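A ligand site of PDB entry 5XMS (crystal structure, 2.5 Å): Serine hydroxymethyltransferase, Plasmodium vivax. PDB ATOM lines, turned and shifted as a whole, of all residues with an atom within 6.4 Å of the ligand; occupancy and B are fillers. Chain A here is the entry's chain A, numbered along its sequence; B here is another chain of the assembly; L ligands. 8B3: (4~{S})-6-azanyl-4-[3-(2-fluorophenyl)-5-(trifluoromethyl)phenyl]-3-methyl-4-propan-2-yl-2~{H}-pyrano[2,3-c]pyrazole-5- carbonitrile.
O of Leu 124 is in hydrogen-bond range of N7 of the ligand (3.1 Å). The backbone carbonyl oxygen of Gly 128 is in hydrogen-bond range of a nitrogen (N7) of the ligand (2.8 Å). A nitrogen (N51) of the ligand lies within hydrogen-bond range of the side-chain carboxylate of Glu 56 of chain B (2.5 Å). OG1 of Thr 183 sits at hydrogen-bond distance from O1 of the ligand (3.1 Å). The side-chain hydroxyl (OG) of Ser 184 is in hydrogen-bond range of a nitrogen (N7) of the ligand (3.5 Å). The side-chain hydroxyl (OG1) of Thr 357 lies within hydrogen-bond range of a nitrogen (N9) of the ligand.
N of Gly 128 is in hydrogen-bond range of O of His 123, at 2.7 Å. N of Tyr 63 of chain B lies within hydrogen-bond range of O of Glu 56 of chain B. The guanidinium group (NH2) of Arg 371 is in hydrogen-bond range of the side-chain hydroxyl (OH) of Tyr 64 of chain B (3.3 Å). The backbone carbonyl oxygen (O) of Gly 127 lies within hydrogen-bond range of the backbone NH (N) of Thr 183, at 2.8 Å. The backbone NH (N) of Asn 356 sits at hydrogen-bond distance from the backbone carbonyl oxygen (O) of Gly 369 (2.7 Å). O of Thr 183 lies within hydrogen-bond range of NH1 of Arg 371 (3.0 Å). The side-chain hydroxyl of Ser 184 lies within hydrogen-bond range of the side-chain amide oxygen of Asn 356. N of Arg 371 sits at hydrogen-bond distance from O of Asn 354 (2.9 Å).
O of Lys 355 sits close to F46 of the ligand (3.3 Å). A fluorine (F47) of the ligand lies close to the backbone carbonyl oxygen (O) of Cys 364 (3.2 Å). Merely in contact with the ligand: Gly 127, His 129, Leu 130, Val 141, Asn 354, Asn 356, Pro 367, Arg 371, Tyr 63 of chain B, Tyr 64 of chain B and Phe 266 of chain B. 19 residues have an atom within 4 Å of the ligand: Leu 124, Gly 127, Gly 128, His 129, Leu 130, Val 141, Thr 183, Ser 184, Asn 354, Lys 355, Asn 356, Thr 357, Cys 364, Pro 367, Arg 371, Glu 56 of chain B, Tyr 63 of chain B, Tyr 64 of chain B and Phe 266 of chain B. The nearest printed residue that does not touch the ligand is Pro 267 of chain B (4.03 Å).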
ATOM      1  N   HIS A 123       5.995  10.376  30.678  1.00  0.00           N
ATOM      2  CA  HIS A 123       6.610  11.446  29.914  1.00  0.00           C
ATOM      3  C   HIS A 123       8.145  11.350  29.963  1.00  0.00           C
ATOM      4  O   HIS A 123       8.713  10.952  30.980  1.00  0.00           O
ATOM      5  CB  HIS A 123       6.133  12.778  30.496  1.00  0.00           C
ATOM      6  CG  HIS A 123       6.400  13.941  29.610  1.00  0.00           C
ATOM      7  ND1 HIS A 123       7.647  14.481  29.454  1.00  0.00           N
ATOM      8  CD2 HIS A 123       5.568  14.687  28.842  1.00  0.00           C
ATOM      9  CE1 HIS A 123       7.591  15.491  28.600  1.00  0.00           C
ATOM     10  NE2 HIS A 123       6.330  15.637  28.216  1.00  0.00           N
ATOM     11  N   LEU A 124       8.794  11.711  28.864  1.00  0.00           N
ATOM     12  CA  LEU A 124      10.257  11.681  28.763  1.00  0.00           C
ATOM     13  C   LEU A 124      10.913  12.507  29.861  1.00  0.00           C
ATOM     14  O   LEU A 124      11.828  12.039  30.541  1.00  0.00           O
ATOM     15  CB  LEU A 124      10.692  12.179  27.378  1.00  0.00           C
ATOM     16  CG  LEU A 124      12.176  12.110  26.970  1.00  0.00           C
ATOM     17  CD1 LEU A 124      12.522  10.793  26.288  1.00  0.00           C
ATOM     18  CD2 LEU A 124      12.505  13.288  26.072  1.00  0.00           C
ATOM     19  N   CYS A 125      10.443  13.753  29.993  1.00  0.00           N
ATOM     20  CA  CYS A 125      10.852  14.679  31.082  1.00  0.00           C
ATOM     21  C   CYS A 125      10.729  14.163  32.520  1.00  0.00           C
ATOM     22  O   CYS A 125      11.481  14.591  33.395  1.00  0.00           O
ATOM     23  CB  CYS A 125      10.150  16.044  30.948  1.00  0.00           C
ATOM     24  SG  CYS A 125      10.526  16.942  29.391  1.00  0.00           S
ATOM     25  N   SER A 126       9.788  13.261  32.778  1.00  0.00           N
ATOM     26  CA  SER A 126       9.635  12.648  34.077  1.00  0.00           C
ATOM     27  C   SER A 126      10.334  11.303  34.201  1.00  0.00           C
ATOM     28  O   SER A 126      10.224  10.662  35.241  1.00  0.00           O
ATOM     29  CB  SER A 126       8.153  12.444  34.407  1.00  0.00           C
ATOM     30  OG  SER A 126       7.376  13.577  34.058  1.00  0.00           O
ATOM     31  N   GLY A 127      11.035  10.862  33.161  1.00  0.00           N
ATOM     32  CA  GLY A 127      11.769   9.584  33.193  1.00  0.00           C
ATOM     33  C   GLY A 127      11.291   8.490  32.237  1.00  0.00           C
ATOM     34  O   GLY A 127      11.841   7.416  32.237  1.00  0.00           O
ATOM     35  N   GLY A 128      10.280   8.775  31.431  1.00  0.00           N
ATOM     36  CA  GLY A 128       9.831   7.830  30.433  1.00  0.00           C
ATOM     37  C   GLY A 128      10.732   7.756  29.208  1.00  0.00           C
ATOM     38  O   GLY A 128      11.586   8.616  28.977  1.00  0.00           O
ATOM     39  N   HIS A 129      10.572   6.689  28.428  1.00  0.00           N
ATOM     40  CA  HIS A 129      11.294   6.569  27.172  1.00  0.00           C
ATOM     41  C   HIS A 129      10.570   7.205  26.026  1.00  0.00           C
ATOM     42  O   HIS A 129       9.383   7.442  26.084  1.00  0.00           O
ATOM     43  CB  HIS A 129      11.637   5.123  26.835  1.00  0.00           C
ATOM     44  CG  HIS A 129      12.749   5.004  25.841  1.00  0.00           C
ATOM     45  ND1 HIS A 129      12.541   4.633  24.541  1.00  0.00           N
ATOM     46  CD2 HIS A 129      14.079   5.281  25.943  1.00  0.00           C
ATOM     47  CE1 HIS A 129      13.679   4.654  23.879  1.00  0.00           C
ATOM     48  NE2 HIS A 129      14.626   5.036  24.706  1.00  0.00           N
ATOM     49  N   LEU A 130      11.330   7.469  24.968  1.00  0.00           N
ATOM     50  CA  LEU A 130      10.793   8.016  23.718  1.00  0.00           C
ATOM     51  C   LEU A 130       9.731   7.105  23.105  1.00  0.00           C
ATOM     52  O   LEU A 130       8.756   7.570  22.554  1.00  0.00           O
ATOM     53  CB  LEU A 130      11.916   8.185  22.692  1.00  0.00           C
ATOM     54  CG  LEU A 130      13.117   9.043  23.064  1.00  0.00           C
ATOM     55  CD1 LEU A 130      14.357   8.556  22.344  1.00  0.00           C
ATOM     56  CD2 LEU A 130      12.848  10.514  22.780  1.00  0.00           C
ATOM     57  N   PHE A 134       6.101   9.487  23.439  1.00  0.00           N
ATOM     58  CA  PHE A 134       6.567  10.857  23.555  1.00  0.00           C
ATOM     59  C   PHE A 134       6.310  11.752  22.336  1.00  0.00           C
ATOM     60  O   PHE A 134       6.698  11.434  21.213  1.00  0.00           O
ATOM     61  CB  PHE A 134       8.048  10.926  23.861  1.00  0.00           C
ATOM     62  CG  PHE A 134       8.527  12.332  24.036  1.00  0.00           C
ATOM     63  CD1 PHE A 134       8.092  13.091  25.123  1.00  0.00           C
ATOM     64  CD2 PHE A 134       9.352  12.918  23.082  1.00  0.00           C
ATOM     65  CE1 PHE A 134       8.483  14.403  25.272  1.00  0.00           C
ATOM     66  CE2 PHE A 134       9.757  14.232  23.241  1.00  0.00           C
ATOM     67  CZ  PHE A 134       9.327  14.984  24.331  1.00  0.00           C
ATOM     68  N   VAL A 141       7.228  13.609  18.252  1.00  0.00           N
ATOM     69  CA  VAL A 141       8.639  13.268  18.264  1.00  0.00           C
ATOM     70  C   VAL A 141       8.894  11.783  18.086  1.00  0.00           C
ATOM     71  O   VAL A 141       9.877  11.393  17.459  1.00  0.00           O
ATOM     72  CB  VAL A 141       9.314  13.748  19.576  1.00  0.00           C
ATOM     73  CG1 VAL A 141      10.785  13.386  19.616  1.00  0.00           C
ATOM     74  CG2 VAL A 141       9.160  15.264  19.709  1.00  0.00           C
ATOM     75  N   THR A 183      13.223   5.031  31.687  1.00  0.00           N
ATOM     76  CA  THR A 183      14.620   5.227  31.277  1.00  0.00           C
ATOM     77  C   THR A 183      15.475   5.882  32.367  1.00  0.00           C
ATOM     78  O   THR A 183      16.618   5.476  32.575  1.00  0.00           O
ATOM     79  CB  THR A 183      14.814   5.859  29.887  1.00  0.00           C
ATOM     80  OG1 THR A 183      15.510   7.110  30.000  1.00  0.00           O
ATOM     81  CG2 THR A 183      13.534   6.064  29.218  1.00  0.00           C
ATOM     82  N   SER A 184      14.911   6.838  33.097  1.00  0.00           N
ATOM     83  CA  SER A 184      15.646   7.472  34.195  1.00  0.00           C
ATOM     84  C   SER A 184      14.837   7.587  35.471  1.00  0.00           C
ATOM     85  O   SER A 184      14.670   8.648  36.020  1.00  0.00           O
ATOM     86  CB  SER A 184      16.207   8.828  33.751  1.00  0.00           C
ATOM     87  OG  SER A 184      15.393   9.418  32.779  1.00  0.00           O
ATOM     88  N   ASN A 354      25.226  11.808  31.692  1.00  0.00           N
ATOM     89  CA  ASN A 354      24.332  12.477  30.765  1.00  0.00           C
ATOM     90  C   ASN A 354      23.447  13.484  31.471  1.00  0.00           C
ATOM     91  O   ASN A 354      22.988  13.258  32.577  1.00  0.00           O
ATOM     92  CB  ASN A 354      23.506  11.463  29.963  1.00  0.00           C
ATOM     93  CG  ASN A 354      22.470  10.731  30.802  1.00  0.00           C
ATOM     94  OD1 ASN A 354      22.731   9.628  31.297  1.00  0.00           O
ATOM     95  ND2 ASN A 354      21.284  11.337  30.968  1.00  0.00           N
ATOM     96  N   LYS A 355      23.220  14.603  30.799  1.00  0.00           N
ATOM     97  CA  LYS A 355      22.263  15.582  31.266  1.00  0.00           C
ATOM     98  C   LYS A 355      20.872  14.950  31.344  1.00  0.00           C
ATOM     99  O   LYS A 355      20.496  14.154  30.524  1.00  0.00           O
ATOM    100  CB  LYS A 355      22.236  16.820  30.364  1.00  0.00           C
ATOM    101  CG  LYS A 355      22.362  16.529  28.878  1.00  0.00           C
ATOM    102  CD  LYS A 355      21.701  17.574  28.005  1.00  0.00           C
ATOM    103  CE  LYS A 355      22.308  17.557  26.606  1.00  0.00           C
ATOM    104  NZ  LYS A 355      21.360  18.003  25.569  1.00  0.00           N
ATOM    105  N   ASN A 356      20.089  15.335  32.339  1.00  0.00           N
ATOM    106  CA  ASN A 356      18.819  14.708  32.551  1.00  0.00           C
ATOM    107  C   ASN A 356      17.849  15.705  33.111  1.00  0.00           C
ATOM    108  O   ASN A 356      18.226  16.546  33.909  1.00  0.00           O
ATOM    109  CB  ASN A 356      18.995  13.501  33.505  1.00  0.00           C
ATOM    110  CG  ASN A 356      17.932  12.437  33.304  1.00  0.00           C
ATOM    111  OD1 ASN A 356      18.161  11.425  32.637  1.00  0.00           O
ATOM    112  ND2 ASN A 356      16.743  12.674  33.853  1.00  0.00           N
ATOM    113  N   THR A 357      16.595  15.614  32.721  1.00  0.00           N
ATOM    114  CA  THR A 357      15.559  16.484  33.259  1.00  0.00           C
ATOM    115  C   THR A 357      15.229  16.139  34.718  1.00  0.00           C
ATOM    116  O   THR A 357      15.542  15.041  35.194  1.00  0.00           O
ATOM    117  CB  THR A 357      14.284  16.426  32.407  1.00  0.00           C
ATOM    118  OG1 THR A 357      13.901  15.068  32.202  1.00  0.00           O
ATOM    119  CG2 THR A 357      14.525  17.081  31.048  1.00  0.00           C
ATOM    120  N   ASP A 363      11.547  22.183  30.300  1.00  0.00           N
ATOM    121  CA  ASP A 363      12.164  22.153  28.973  1.00  0.00           C
ATOM    122  C   ASP A 363      13.267  21.100  28.845  1.00  0.00           C
ATOM    123  O   ASP A 363      14.096  20.929  29.743  1.00  0.00           O
ATOM    124  CB  ASP A 363      12.709  23.547  28.613  1.00  0.00           C
ATOM    125  CG  ASP A 363      12.814  23.799  27.094  1.00  0.00           C
ATOM    126  OD1 ASP A 363      12.238  23.047  26.266  1.00  0.00           O
ATOM    127  OD2 ASP A 363      13.497  24.772  26.719  1.00  0.00           O
ATOM    128  N   CYS A 364      13.287  20.425  27.702  1.00  0.00           N
ATOM    129  CA  CYS A 364      14.381  19.496  27.323  1.00  0.00           C
ATOM    130  C   CYS A 364      15.609  20.244  26.763  1.00  0.00           C
ATOM    131  O   CYS A 364      16.555  19.628  26.262  1.00  0.00           O
ATOM    132  CB  CYS A 364      13.870  18.454  26.333  1.00  0.00           C
ATOM    133  SG  CYS A 364      12.669  17.365  27.104  1.00  0.00           S
ATOM    134  N   VAL A 365      15.550  21.572  26.848  1.00  0.00           N
ATOM    135  CA  VAL A 365      16.663  22.473  26.623  1.00  0.00           C
ATOM    136  C   VAL A 365      16.891  23.034  28.018  1.00  0.00           C
ATOM    137  O   VAL A 365      15.954  23.483  28.668  1.00  0.00           O
ATOM    138  CB  VAL A 365      16.305  23.622  25.644  1.00  0.00           C
ATOM    139  CG1 VAL A 365      17.538  24.070  24.875  1.00  0.00           C
ATOM    140  CG2 VAL A 365      15.209  23.231  24.664  1.00  0.00           C
ATOM    141  N   SER A 366      18.124  22.986  28.489  1.00  0.00           N
ATOM    142  CA  SER A 366      18.448  23.442  29.839  1.00  0.00           C
ATOM    143  C   SER A 366      17.943  22.539  31.005  1.00  0.00           C
ATOM    144  O   SER A 366      17.508  23.058  32.032  1.00  0.00           O
ATOM    145  CB  SER A 366      17.964  24.894  30.038  1.00  0.00           C
ATOM    146  OG  SER A 366      18.776  25.573  30.986  1.00  0.00           O
ATOM    147  N   PRO A 367      18.028  21.193  30.861  1.00  0.00           N
ATOM    148  CA  PRO A 367      17.686  20.357  32.015  1.00  0.00           C
ATOM    149  C   PRO A 367      18.599  20.603  33.225  1.00  0.00           C
ATOM    150  O   PRO A 367      19.799  20.891  33.063  1.00  0.00           O
ATOM    151  CB  PRO A 367      17.888  18.943  31.482  1.00  0.00           C
ATOM    152  CG  PRO A 367      18.949  19.090  30.483  1.00  0.00           C
ATOM    153  CD  PRO A 367      18.514  20.320  29.760  1.00  0.00           C
ATOM    154  N   GLY A 369      19.561  18.509  35.647  1.00  0.00           N
ATOM    155  CA  GLY A 369      20.196  17.376  36.275  1.00  0.00           C
ATOM    156  C   GLY A 369      21.152  16.587  35.422  1.00  0.00           C
ATOM    157  O   GLY A 369      21.338  16.845  34.230  1.00  0.00           O
ATOM    158  N   ARG A 371      22.321  12.255  35.191  1.00  0.00           N
ATOM    159  CA  ARG A 371      21.998  10.941  35.619  1.00  0.00           C
ATOM    160  C   ARG A 371      23.260  10.102  35.609  1.00  0.00           C
ATOM    161  O   ARG A 371      23.988  10.086  34.636  1.00  0.00           O
ATOM    162  CB  ARG A 371      20.943  10.351  34.691  1.00  0.00           C
ATOM    163  CG  ARG A 371      20.519   8.945  35.026  1.00  0.00           C
ATOM    164  CD  ARG A 371      19.736   8.358  33.875  1.00  0.00           C
ATOM    165  NE  ARG A 371      20.584   8.042  32.740  1.00  0.00           N
ATOM    166  CZ  ARG A 371      20.189   7.425  31.631  1.00  0.00           C
ATOM    167  NH1 ARG A 371      18.956   7.002  31.483  1.00  0.00           N
ATOM    168  NH2 ARG A 371      21.060   7.206  30.648  1.00  0.00           N
ATOM    169  N   GLU B  56      23.076   8.263  20.955  1.00  0.00           N
ATOM    170  CA  GLU B  56      21.872   8.855  20.424  1.00  0.00           C
ATOM    171  C   GLU B  56      22.108  10.225  19.818  1.00  0.00           C
ATOM    172  O   GLU B  56      22.727  11.070  20.418  1.00  0.00           O
ATOM    173  CB  GLU B  56      20.825   8.947  21.517  1.00  0.00           C
ATOM    174  CG  GLU B  56      20.037   7.656  21.654  1.00  0.00           C
ATOM    175  CD  GLU B  56      19.427   7.491  23.010  1.00  0.00           C
ATOM    176  OE1 GLU B  56      20.211   7.398  23.950  1.00  0.00           O
ATOM    177  OE2 GLU B  56      18.190   7.464  23.134  1.00  0.00           O
ATOM    178  N   TYR B  63      23.599  13.361  22.071  1.00  0.00           N
ATOM    179  CA  TYR B  63      23.029  13.643  23.371  1.00  0.00           C
ATOM    180  C   TYR B  63      24.099  13.552  24.423  1.00  0.00           C
ATOM    181  O   TYR B  63      24.133  14.374  25.322  1.00  0.00           O
ATOM    182  CB  TYR B  63      21.783  12.766  23.671  1.00  0.00           C
ATOM    183  CG  TYR B  63      20.561  13.454  23.117  1.00  0.00           C
ATOM    184  CD1 TYR B  63      19.912  14.418  23.860  1.00  0.00           C
ATOM    185  CD2 TYR B  63      20.169  13.259  21.810  1.00  0.00           C
ATOM    186  CE1 TYR B  63      18.853  15.132  23.325  1.00  0.00           C
ATOM    187  CE2 TYR B  63      19.110  13.969  21.266  1.00  0.00           C
ATOM    188  CZ  TYR B  63      18.463  14.909  22.043  1.00  0.00           C
ATOM    189  OH  TYR B  63      17.396  15.620  21.545  1.00  0.00           O
ATOM    190  N   TYR B  64      24.983  12.561  24.302  1.00  0.00           N
ATOM    191  CA  TYR B  64      26.053  12.341  25.274  1.00  0.00           C
ATOM    192  C   TYR B  64      27.383  12.747  24.697  1.00  0.00           C
ATOM    193  O   TYR B  64      27.514  12.863  23.490  1.00  0.00           O
ATOM    194  CB  TYR B  64      26.161  10.863  25.640  1.00  0.00           C
ATOM    195  CG  TYR B  64      24.906  10.234  26.154  1.00  0.00           C
ATOM    196  CD1 TYR B  64      23.699  10.901  26.134  1.00  0.00           C
ATOM    197  CD2 TYR B  64      24.926   8.952  26.665  1.00  0.00           C
ATOM    198  CE1 TYR B  64      22.560  10.312  26.598  1.00  0.00           C
ATOM    199  CE2 TYR B  64      23.783   8.342  27.150  1.00  0.00           C
ATOM    200  CZ  TYR B  64      22.601   9.028  27.097  1.00  0.00           C
ATOM    201  OH  TYR B  64      21.448   8.441  27.560  1.00  0.00           O
ATOM    202  N   PHE B 266      16.081   8.660  13.814  1.00  0.00           N
ATOM    203  CA  PHE B 266      16.087   9.001  15.244  1.00  0.00           C
ATOM    204  C   PHE B 266      15.634  10.423  15.445  1.00  0.00           C
ATOM    205  O   PHE B 266      16.081  11.286  14.717  1.00  0.00           O
ATOM    206  CB  PHE B 266      17.473   8.817  15.840  1.00  0.00           C
ATOM    207  CG  PHE B 266      17.587   9.350  17.245  1.00  0.00           C
ATOM    208  CD1 PHE B 266      17.261   8.551  18.335  1.00  0.00           C
ATOM    209  CD2 PHE B 266      17.986  10.678  17.475  1.00  0.00           C
ATOM    210  CE1 PHE B 266      17.361   9.033  19.621  1.00  0.00           C
ATOM    211  CE2 PHE B 266      18.102  11.167  18.779  1.00  0.00           C
ATOM    212  CZ  PHE B 266      17.793  10.345  19.846  1.00  0.00           C
ATOM    213  N   PRO B 267      14.750  10.723  16.422  1.00  0.00           N
ATOM    214  CA  PRO B 267      14.260   9.726  17.377  1.00  0.00           C
ATOM    215  C   PRO B 267      12.900   9.107  17.066  1.00  0.00           C
ATOM    216  O   PRO B 267      12.297   8.502  17.956  1.00  0.00           O
ATOM    217  CB  PRO B 267      14.154  10.535  18.672  1.00  0.00           C
ATOM    218  CG  PRO B 267      13.658  11.851  18.190  1.00  0.00           C
ATOM    219  CD  PRO B 267      14.251  12.071  16.808  1.00  0.00           C
HETATM  220  C2  8B3 L   1      14.851  10.108  28.741  1.00  0.00           C
HETATM  221  C3  8B3 L   1      15.719  11.144  28.703  1.00  0.00           C
HETATM  222  C4  8B3 L   1      16.809  11.292  27.656  1.00  0.00           C
HETATM  223  C5  8B3 L   1      16.721  10.198  26.627  1.00  0.00           C
HETATM  224  C6  8B3 L   1      15.735   9.113  26.699  1.00  0.00           C
HETATM  225  N11 8B3 L   1      15.810   8.247  25.691  1.00  0.00           N
HETATM  226  C12 8B3 L   1      18.567  10.565  24.669  1.00  0.00           C
HETATM  227  C13 8B3 L   1      18.139  11.136  28.409  1.00  0.00           C
HETATM  228  C14 8B3 L   1      19.378  11.446  27.562  1.00  0.00           C
HETATM  229  C15 8B3 L   1      16.670  12.651  26.981  1.00  0.00           C
HETATM  230  C16 8B3 L   1      17.202  13.803  27.580  1.00  0.00           C
HETATM  231  C17 8B3 L   1      17.078  15.060  27.011  1.00  0.00           C
HETATM  232  C18 8B3 L   1      16.428  15.188  25.798  1.00  0.00           C
HETATM  233  C19 8B3 L   1      15.905  14.081  25.165  1.00  0.00           C
HETATM  234  C20 8B3 L   1      16.013  12.820  25.749  1.00  0.00           C
HETATM  235  F50 8B3 L   1      16.394  12.478  22.916  1.00  0.00           F
HETATM  236  C39 8B3 L   1      15.503  13.486  22.783  1.00  0.00           C
HETATM  237  C40 8B3 L   1      14.865  13.677  21.571  1.00  0.00           C
HETATM  238  C41 8B3 L   1      13.949  14.702  21.431  1.00  0.00           C
HETATM  239  C42 8B3 L   1      13.670  15.528  22.518  1.00  0.00           C
HETATM  240  C43 8B3 L   1      14.290  15.314  23.743  1.00  0.00           C
HETATM  241  C32 8B3 L   1      15.213  14.289  23.870  1.00  0.00           C
HETATM  242  C33 8B3 L   1      17.648  16.304  27.663  1.00  0.00           C
HETATM  243  F48 8B3 L   1      16.690  17.049  28.112  1.00  0.00           F
HETATM  244  F47 8B3 L   1      18.282  17.035  26.763  1.00  0.00           F
HETATM  245  F46 8B3 L   1      18.395  16.021  28.722  1.00  0.00           F
HETATM  246  C34 8B3 L   1      18.303   9.755  29.081  1.00  0.00           C
HETATM  247  C8  8B3 L   1      15.709  12.042  29.578  1.00  0.00           C
HETATM  248  N9  8B3 L   1      15.721  12.892  30.397  1.00  0.00           N
HETATM  249  N7  8B3 L   1      13.919   9.990  29.672  1.00  0.00           N
HETATM  250  C10 8B3 L   1      17.436   9.852  25.383  1.00  0.00           C
HETATM  251  N51 8B3 L   1      16.871   8.728  24.907  1.00  0.00           N
HETATM  252  O1  8B3 L   1      14.865   9.067  27.746  1.00  0.00           O
